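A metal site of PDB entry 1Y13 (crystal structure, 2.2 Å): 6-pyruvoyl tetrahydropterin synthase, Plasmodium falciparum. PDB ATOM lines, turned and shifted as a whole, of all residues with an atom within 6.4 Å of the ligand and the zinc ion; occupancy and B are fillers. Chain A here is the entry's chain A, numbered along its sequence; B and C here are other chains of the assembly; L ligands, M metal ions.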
ATOM      1  N   HIS A  37       6.562  19.091  16.670  1.00  0.00           N
ATOM      2  CA  HIS A  37       7.118  19.048  18.022  1.00  0.00           C
ATOM      3  C   HIS A  37       8.004  17.803  18.171  1.00  0.00           C
ATOM      4  O   HIS A  37       8.017  16.937  17.298  1.00  0.00           O
ATOM      5  CB  HIS A  37       5.975  19.026  19.079  1.00  0.00           C
ATOM      6  CG  HIS A  37       5.488  17.645  19.419  1.00  0.00           C
ATOM      7  ND1 HIS A  37       5.532  17.133  20.700  1.00  0.00           N
ATOM      8  CD2 HIS A  37       4.935  16.676  18.643  1.00  0.00           C
ATOM      9  CE1 HIS A  37       5.012  15.914  20.701  1.00  0.00           C
ATOM     10  NE2 HIS A  37       4.648  15.618  19.473  1.00  0.00           N
ATOM     11  N   PHE A  38       8.732  17.729  19.279  1.00  0.00           N
ATOM     12  CA  PHE A  38       9.264  16.457  19.704  1.00  0.00           C
ATOM     13  C   PHE A  38       9.309  16.471  21.216  1.00  0.00           C
ATOM     14  O   PHE A  38       9.528  17.505  21.832  1.00  0.00           O
ATOM     15  CB  PHE A  38      10.640  16.141  19.058  1.00  0.00           C
ATOM     16  CG  PHE A  38      11.728  17.129  19.393  1.00  0.00           C
ATOM     17  CD1 PHE A  38      12.479  16.977  20.534  1.00  0.00           C
ATOM     18  CD2 PHE A  38      12.003  18.202  18.549  1.00  0.00           C
ATOM     19  CE1 PHE A  38      13.504  17.899  20.852  1.00  0.00           C
ATOM     20  CE2 PHE A  38      13.007  19.101  18.838  1.00  0.00           C
ATOM     21  CZ  PHE A  38      13.752  18.973  19.996  1.00  0.00           C
ATOM     22  N   ILE A  39       9.029  15.317  21.807  1.00  0.00           N
ATOM     23  CA  ILE A  39       9.184  15.171  23.249  1.00  0.00           C
ATOM     24  C   ILE A  39      10.628  14.926  23.684  1.00  0.00           C
ATOM     25  O   ILE A  39      11.376  14.195  23.040  1.00  0.00           O
ATOM     26  CB  ILE A  39       8.186  14.139  23.790  1.00  0.00           C
ATOM     27  CG1 ILE A  39       6.843  14.856  24.008  1.00  0.00           C
ATOM     28  CG2 ILE A  39       8.696  13.519  25.086  1.00  0.00           C
ATOM     29  CD1 ILE A  39       5.649  13.977  23.862  1.00  0.00           C
ATOM     30  N   GLU A  46      12.926  12.149  21.159  1.00  0.00           N
ATOM     31  CA  GLU A  46      12.422  11.512  19.936  1.00  0.00           C
ATOM     32  C   GLU A  46      12.653  12.454  18.752  1.00  0.00           C
ATOM     33  O   GLU A  46      12.936  13.639  18.927  1.00  0.00           O
ATOM     34  CB  GLU A  46      10.921  11.145  20.057  1.00  0.00           C
ATOM     35  CG  GLU A  46      10.000  12.357  20.072  1.00  0.00           C
ATOM     36  CD  GLU A  46       8.556  12.055  20.483  1.00  0.00           C
ATOM     37  OE1 GLU A  46       8.187  10.875  20.664  1.00  0.00           O
ATOM     38  OE2 GLU A  46       7.782  13.033  20.614  1.00  0.00           O
ATOM     39  N   HIS A  49       8.455  15.413  14.568  1.00  0.00           N
ATOM     40  CA  HIS A  49       7.279  14.967  13.827  1.00  0.00           C
ATOM     41  C   HIS A  49       6.160  15.984  14.084  1.00  0.00           C
ATOM     42  O   HIS A  49       6.442  17.110  14.470  1.00  0.00           O
ATOM     43  CB  HIS A  49       6.868  13.538  14.211  1.00  0.00           C
ATOM     44  CG  HIS A  49       6.516  13.407  15.657  1.00  0.00           C
ATOM     45  ND1 HIS A  49       7.455  13.530  16.665  1.00  0.00           N
ATOM     46  CD2 HIS A  49       5.321  13.214  16.267  1.00  0.00           C
ATOM     47  CE1 HIS A  49       6.854  13.403  17.836  1.00  0.00           C
ATOM     48  NE2 HIS A  49       5.560  13.219  17.625  1.00  0.00           N
ATOM     49  N   GLY A  50       4.911  15.610  13.843  1.00  0.00           N
ATOM     50  CA  GLY A  50       3.814  16.548  14.012  1.00  0.00           C
ATOM     51  C   GLY A  50       2.480  15.889  14.208  1.00  0.00           C
ATOM     52  O   GLY A  50       2.361  14.689  14.090  1.00  0.00           O
ATOM     53  N   HIS A  51       1.476  16.710  14.513  1.00  0.00           N
ATOM     54  CA  HIS A  51       0.121  16.257  14.790  1.00  0.00           C
ATOM     55  C   HIS A  51      -0.911  17.292  14.374  1.00  0.00           C
ATOM     56  O   HIS A  51      -0.637  18.485  14.365  1.00  0.00           O
ATOM     57  CB  HIS A  51      -0.066  15.983  16.291  1.00  0.00           C
ATOM     58  CG  HIS A  51       0.838  14.920  16.812  1.00  0.00           C
ATOM     59  ND1 HIS A  51       0.704  13.605  16.444  1.00  0.00           N
ATOM     60  CD2 HIS A  51       1.902  14.976  17.648  1.00  0.00           C
ATOM     61  CE1 HIS A  51       1.647  12.883  17.033  1.00  0.00           C
ATOM     62  NE2 HIS A  51       2.388  13.707  17.765  1.00  0.00           N
ATOM     63  N   TYR A  53      -3.679  18.543  16.288  1.00  0.00           N
ATOM     64  CA  TYR A  53      -4.231  18.504  17.633  1.00  0.00           C
ATOM     65  C   TYR A  53      -5.638  19.037  17.577  1.00  0.00           C
ATOM     66  O   TYR A  53      -5.924  19.968  16.815  1.00  0.00           O
ATOM     67  CB  TYR A  53      -3.448  19.346  18.599  1.00  0.00           C
ATOM     68  CG  TYR A  53      -2.038  18.913  18.874  1.00  0.00           C
ATOM     69  CD1 TYR A  53      -0.971  19.379  18.073  1.00  0.00           C
ATOM     70  CD2 TYR A  53      -1.745  18.111  19.984  1.00  0.00           C
ATOM     71  CE1 TYR A  53       0.345  19.018  18.371  1.00  0.00           C
ATOM     72  CE2 TYR A  53      -0.435  17.758  20.280  1.00  0.00           C
ATOM     73  CZ  TYR A  53       0.618  18.225  19.477  1.00  0.00           C
ATOM     74  OH  TYR A  53       1.904  17.854  19.774  1.00  0.00           O
ATOM     75  N   SER A 133       6.433  19.381  25.455  1.00  0.00           N
ATOM     76  CA  SER A 133       5.345  19.514  24.499  1.00  0.00           C
ATOM     77  C   SER A 133       4.461  18.258  24.463  1.00  0.00           C
ATOM     78  O   SER A 133       4.112  17.750  23.398  1.00  0.00           O
ATOM     79  CB  SER A 133       5.869  19.865  23.088  1.00  0.00           C
ATOM     80  OG  SER A 133       6.791  18.884  22.636  1.00  0.00           O
ATOM     81  N   SER A 134       4.101  17.740  25.627  1.00  0.00           N
ATOM     82  CA  SER A 134       3.184  16.625  25.711  1.00  0.00           C
ATOM     83  C   SER A 134       1.785  17.178  25.602  1.00  0.00           C
ATOM     84  O   SER A 134       1.528  18.359  25.872  1.00  0.00           O
ATOM     85  CB  SER A 134       3.361  15.881  27.045  1.00  0.00           C
ATOM     86  OG  SER A 134       2.915  16.673  28.143  1.00  0.00           O
ATOM     87  N   THR A 135       0.867  16.313  25.215  1.00  0.00           N
ATOM     88  CA  THR A 135      -0.550  16.612  25.069  1.00  0.00           C
ATOM     89  C   THR A 135      -1.162  17.088  26.388  1.00  0.00           C
ATOM     90  O   THR A 135      -1.924  18.063  26.399  1.00  0.00           O
ATOM     91  CB  THR A 135      -1.266  15.338  24.493  1.00  0.00           C
ATOM     92  OG1 THR A 135      -0.492  14.839  23.383  1.00  0.00           O
ATOM     93  CG2 THR A 135      -2.612  15.666  23.964  1.00  0.00           C
ATOM     94  N   GLU A 136      -0.818  16.415  27.494  1.00  0.00           N
ATOM     95  CA  GLU A 136      -1.159  16.854  28.853  1.00  0.00           C
ATOM     96  C   GLU A 136      -0.744  18.295  29.136  1.00  0.00           C
ATOM     97  O   GLU A 136      -1.555  19.100  29.562  1.00  0.00           O
ATOM     98  CB  GLU A 136      -0.531  15.947  29.925  1.00  0.00           C
ATOM     99  CG  GLU A 136      -1.073  14.515  29.984  1.00  0.00           C
ATOM    100  CD  GLU A 136      -0.220  13.549  29.179  1.00  0.00           C
ATOM    101  OE1 GLU A 136       0.232  13.933  28.072  1.00  0.00           O
ATOM    102  OE2 GLU A 136       0.020  12.408  29.662  1.00  0.00           O
ATOM    103  N   GLU A 169      -4.016  14.321  20.439  1.00  0.00           N
ATOM    104  CA  GLU A 169      -2.864  14.432  19.532  1.00  0.00           C
ATOM    105  C   GLU A 169      -3.108  13.688  18.235  1.00  0.00           C
ATOM    106  O   GLU A 169      -2.472  13.953  17.231  1.00  0.00           O
ATOM    107  CB  GLU A 169      -1.551  14.018  20.201  1.00  0.00           C
ATOM    108  CG  GLU A 169      -1.299  12.530  20.338  1.00  0.00           C
ATOM    109  CD  GLU A 169       0.191  12.205  20.585  1.00  0.00           C
ATOM    110  OE1 GLU A 169       0.951  13.064  21.101  1.00  0.00           O
ATOM    111  OE2 GLU A 169       0.605  11.066  20.232  1.00  0.00           O
ATOM    112  N   GLN A 173      -5.657   9.003  20.643  1.00  0.00           N
ATOM    113  CA  GLN A 173      -5.078   9.318  21.958  1.00  0.00           C
ATOM    114  C   GLN A 173      -5.326  10.752  22.417  1.00  0.00           C
ATOM    115  O   GLN A 173      -5.056  11.703  21.691  1.00  0.00           O
ATOM    116  CB  GLN A 173      -3.588   8.955  22.018  1.00  0.00           C
ATOM    117  CG  GLN A 173      -2.799   9.245  20.740  1.00  0.00           C
ATOM    118  CD  GLN A 173      -1.516   8.414  20.634  1.00  0.00           C
ATOM    119  OE1 GLN A 173      -1.537   7.193  20.791  1.00  0.00           O
ATOM    120  NE2 GLN A 173      -0.403   9.077  20.357  1.00  0.00           N
ATOM    121  N   VAL B  24      -5.591  10.471  30.701  1.00  0.00           N
ATOM    122  CA  VAL B  24      -5.264  10.132  29.318  1.00  0.00           C
ATOM    123  C   VAL B  24      -6.129   8.955  28.907  1.00  0.00           C
ATOM    124  O   VAL B  24      -6.482   8.127  29.730  1.00  0.00           O
ATOM    125  CB  VAL B  24      -3.753   9.816  29.089  1.00  0.00           C
ATOM    126  CG1 VAL B  24      -2.923  11.094  29.128  1.00  0.00           C
ATOM    127  CG2 VAL B  24      -3.228   8.829  30.113  1.00  0.00           C
ATOM    128  N   GLY B  67       6.469  14.538  31.720  1.00  0.00           N
ATOM    129  CA  GLY B  67       5.435  15.258  30.972  1.00  0.00           C
ATOM    130  C   GLY B  67       4.130  14.518  30.726  1.00  0.00           C
ATOM    131  O   GLY B  67       3.228  15.055  30.086  1.00  0.00           O
ATOM    132  N   TYR B  68       4.036  13.287  31.243  1.00  0.00           N
ATOM    133  CA  TYR B  68       2.918  12.387  30.944  1.00  0.00           C
ATOM    134  C   TYR B  68       2.140  12.034  32.191  1.00  0.00           C
ATOM    135  O   TYR B  68       2.702  11.991  33.270  1.00  0.00           O
ATOM    136  CB  TYR B  68       3.429  11.054  30.413  1.00  0.00           C
ATOM    137  CG  TYR B  68       4.194  11.082  29.139  1.00  0.00           C
ATOM    138  CD1 TYR B  68       3.958  12.074  28.171  1.00  0.00           C
ATOM    139  CD2 TYR B  68       5.134  10.100  28.861  1.00  0.00           C
ATOM    140  CE1 TYR B  68       4.657  12.092  26.974  1.00  0.00           C
ATOM    141  CE2 TYR B  68       5.855  10.105  27.647  1.00  0.00           C
ATOM    142  CZ  TYR B  68       5.609  11.111  26.717  1.00  0.00           C
ATOM    143  OH  TYR B  68       6.309  11.143  25.528  1.00  0.00           O
ATOM    144  N   VAL B  69       0.840  11.728  32.037  1.00  0.00           N
ATOM    145  CA  VAL B  69       0.149  10.950  33.077  1.00  0.00           C
ATOM    146  C   VAL B  69       0.783   9.537  33.055  1.00  0.00           C
ATOM    147  O   VAL B  69       1.225   9.029  34.086  1.00  0.00           O
ATOM    148  CB  VAL B  69      -1.391  10.885  32.879  1.00  0.00           C
ATOM    149  CG1 VAL B  69      -2.034   9.980  33.930  1.00  0.00           C
ATOM    150  CG2 VAL B  69      -1.996  12.246  32.972  1.00  0.00           C
ATOM    151  N   ILE B  70       0.828   8.961  31.851  1.00  0.00           N
ATOM    152  CA  ILE B  70       1.552   7.733  31.507  1.00  0.00           C
ATOM    153  C   ILE B  70       1.684   7.738  29.978  1.00  0.00           C
ATOM    154  O   ILE B  70       0.825   8.299  29.287  1.00  0.00           O
ATOM    155  CB  ILE B  70       0.822   6.455  32.024  1.00  0.00           C
ATOM    156  CG1 ILE B  70       1.658   5.202  31.825  1.00  0.00           C
ATOM    157  CG2 ILE B  70      -0.577   6.280  31.388  1.00  0.00           C
ATOM    158  CD1 ILE B  70       1.272   4.062  32.760  1.00  0.00           C
ATOM    159  N   ASP B  71       2.744   7.131  29.436  1.00  0.00           N
ATOM    160  CA  ASP B  71       2.961   7.092  27.991  1.00  0.00           C
ATOM    161  C   ASP B  71       1.771   6.420  27.269  1.00  0.00           C
ATOM    162  O   ASP B  71       1.335   5.348  27.663  1.00  0.00           O
ATOM    163  CB  ASP B  71       4.260   6.348  27.681  1.00  0.00           C
ATOM    164  CG  ASP B  71       4.819   6.653  26.290  1.00  0.00           C
ATOM    165  OD1 ASP B  71       4.061   6.753  25.297  1.00  0.00           O
ATOM    166  OD2 ASP B  71       6.069   6.789  26.189  1.00  0.00           O
ATOM    167  N   PHE B  72       1.255   7.071  26.212  1.00  0.00           N
ATOM    168  CA  PHE B  72       0.166   6.511  25.402  1.00  0.00           C
ATOM    169  C   PHE B  72       0.544   5.121  24.908  1.00  0.00           C
ATOM    170  O   PHE B  72      -0.293   4.227  24.887  1.00  0.00           O
ATOM    171  CB  PHE B  72      -0.180   7.377  24.178  1.00  0.00           C
ATOM    172  CG  PHE B  72      -0.910   8.660  24.494  1.00  0.00           C
ATOM    173  CD1 PHE B  72      -2.051   8.663  25.285  1.00  0.00           C
ATOM    174  CD2 PHE B  72      -0.483   9.870  23.929  1.00  0.00           C
ATOM    175  CE1 PHE B  72      -2.730   9.848  25.558  1.00  0.00           C
ATOM    176  CE2 PHE B  72      -1.161  11.053  24.182  1.00  0.00           C
ATOM    177  CZ  PHE B  72      -2.292  11.043  25.005  1.00  0.00           C
ATOM    178  N   SER B  73       1.804   4.945  24.507  1.00  0.00           N
ATOM    179  CA  SER B  73       2.283   3.667  23.925  1.00  0.00           C
ATOM    180  C   SER B  73       2.160   2.468  24.880  1.00  0.00           C
ATOM    181  O   SER B  73       1.913   1.342  24.426  1.00  0.00           O
ATOM    182  CB  SER B  73       3.722   3.795  23.437  1.00  0.00           C
ATOM    183  OG  SER B  73       4.607   4.005  24.519  1.00  0.00           O
ATOM    184  N   ASN C  34       2.716  10.221  11.455  1.00  0.00           N
ATOM    185  CA  ASN C  34       2.674  11.542  12.080  1.00  0.00           C
ATOM    186  C   ASN C  34       3.966  12.250  11.721  1.00  0.00           C
ATOM    187  O   ASN C  34       5.029  11.878  12.241  1.00  0.00           O
ATOM    188  CB  ASN C  34       2.496  11.435  13.609  1.00  0.00           C
ATOM    189  CG  ASN C  34       1.255  10.644  13.994  1.00  0.00           C
ATOM    190  OD1 ASN C  34       0.336  10.453  13.199  1.00  0.00           O
ATOM    191  ND2 ASN C  34       1.232  10.169  15.212  1.00  0.00           N
ATOM    192  N   HIS C  88       6.904   9.556  12.079  1.00  0.00           N
ATOM    193  CA  HIS C  88       7.821  10.256  12.975  1.00  0.00           C
ATOM    194  C   HIS C  88       9.048  10.879  12.328  1.00  0.00           C
ATOM    195  O   HIS C  88      10.140  10.778  12.864  1.00  0.00           O
ATOM    196  CB  HIS C  88       8.250   9.363  14.129  1.00  0.00           C
ATOM    197  CG  HIS C  88       7.337   9.456  15.302  1.00  0.00           C
ATOM    198  ND1 HIS C  88       7.734   9.970  16.523  1.00  0.00           N
ATOM    199  CD2 HIS C  88       6.020   9.147  15.442  1.00  0.00           C
ATOM    200  CE1 HIS C  88       6.714   9.948  17.358  1.00  0.00           C
ATOM    201  NE2 HIS C  88       5.665   9.456  16.726  1.00  0.00           N
HETATM  202  N1  LIG L   1       2.169  10.098  25.854  1.00  0.00           N
HETATM  203  N2  LIG L   1       0.821  10.748  27.631  1.00  0.00           N
HETATM  204  C1  LIG L   1       1.457  11.058  26.469  1.00  0.00           C
HETATM  205  N3  LIG L   1       1.414  12.285  25.901  1.00  0.00           N
HETATM  206  C2  LIG L   1       2.826  11.665  24.023  1.00  0.00           C
HETATM  207  C3  LIG L   1       2.842  10.345  24.683  1.00  0.00           C
HETATM  208  N4  LIG L   1       3.569   9.351  24.094  1.00  0.00           N
HETATM  209  C4  LIG L   1       4.254   9.534  22.944  1.00  0.00           C
HETATM  210  C5  LIG L   1       4.224  10.758  22.306  1.00  0.00           C
HETATM  211  N5  LIG L   1       3.524  11.781  22.873  1.00  0.00           N
HETATM  212  C6  LIG L   1       4.992  10.977  21.016  1.00  0.00           C
HETATM  213  O1  LIG L   1       5.409  12.388  20.838  1.00  0.00           O
HETATM  214  C7  LIG L   1       4.232  10.489  19.740  1.00  0.00           C
HETATM  215  O2  LIG L   1       3.481  11.564  19.130  1.00  0.00           O
HETATM  216  C8  LIG L   1       3.288   9.281  19.914  1.00  0.00           C
HETATM  217 ZN    ZN M   1       4.111  13.407  19.174  1.00  0.00          ZN
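OE2 of Glu 46 sits close to O1 of the ligand (2.5 Å). The side-chain carboxylate (OE2) of Glu 136 is in hydrogen-bond range of a nitrogen (N2) of the ligand. A nitrogen (N2) of the ligand is in hydrogen-bond range of the backbone carbonyl oxygen (O) of Ile 70 of chain B (3.0 Å). OE2 of Glu 169 sits close to O2 of the ligand (3.1 Å). The backbone NH of Phe 72 of chain B lies within hydrogen-bond range of a nitrogen (N1) of the ligand, at 3.2 Å.
ND1 of His 51 lies close to O of Glu 169 (3.3 Å). OG of Ser 133 sits at hydrogen-bond distance from ND1 of His 37. The side-chain carboxylate of Glu 46 lies within hydrogen-bond range of the backbone NH of Ile 39 (2.9 Å). The backbone NH (N) of Val 69 of chain B lies within hydrogen-bond range of the side-chain carboxylate (OE2) of Glu 136 (2.6 Å). OD1 of Asp 71 of chain B lies within hydrogen-bond range of OG of Ser 73 of chain B. The side-chain carboxylate of Glu 169 lies within hydrogen-bond range of the side-chain hydroxyl of Thr 135. The backbone NH (N) of His 88 of chain C lies within hydrogen-bond range of the backbone carbonyl oxygen (O) of Asn 34 of chain C, 3.0 Å away.
A nitrogen (N4) of the ligand lies close to the side-chain carboxylate of Asp 71 of chain B. Residues that only touch the ligand: Tyr 68 of chain B (3.2 Å), Ile 39 (3.2 Å), His 88 of chain C (3.5 Å) and Gln 173 (3.7 Å). Hydrophobic or aromatic side chains within 4 Å of the ligand: His 37, Ile 39, His 49, His 51, Tyr 68 of chain B, Phe 72 of chain B and His 88 of chain C. Of the 24 residues printed, 13 come within 4 Å of the ligand. The nearest printed residue that does not touch the ligand is Val 24 of chain B (4.05 Å).
OE2 of Glu 46 touches the zinc ion, at 3.96 Å. OE1 of Glu 169 touches the zinc ion (3.7 Å). The nearest printed residue that does not touch the zinc ion is His 88 of chain C (4.7 Å).
The zinc ion is bound by O2 of the ligand (1.9 Å), NE2 of His 49 (2.1 Å), NE2 of His 51 (2.2 Å), NE2 of His 37 (2.3 Å) and O1 of the ligand (2.3 Å).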
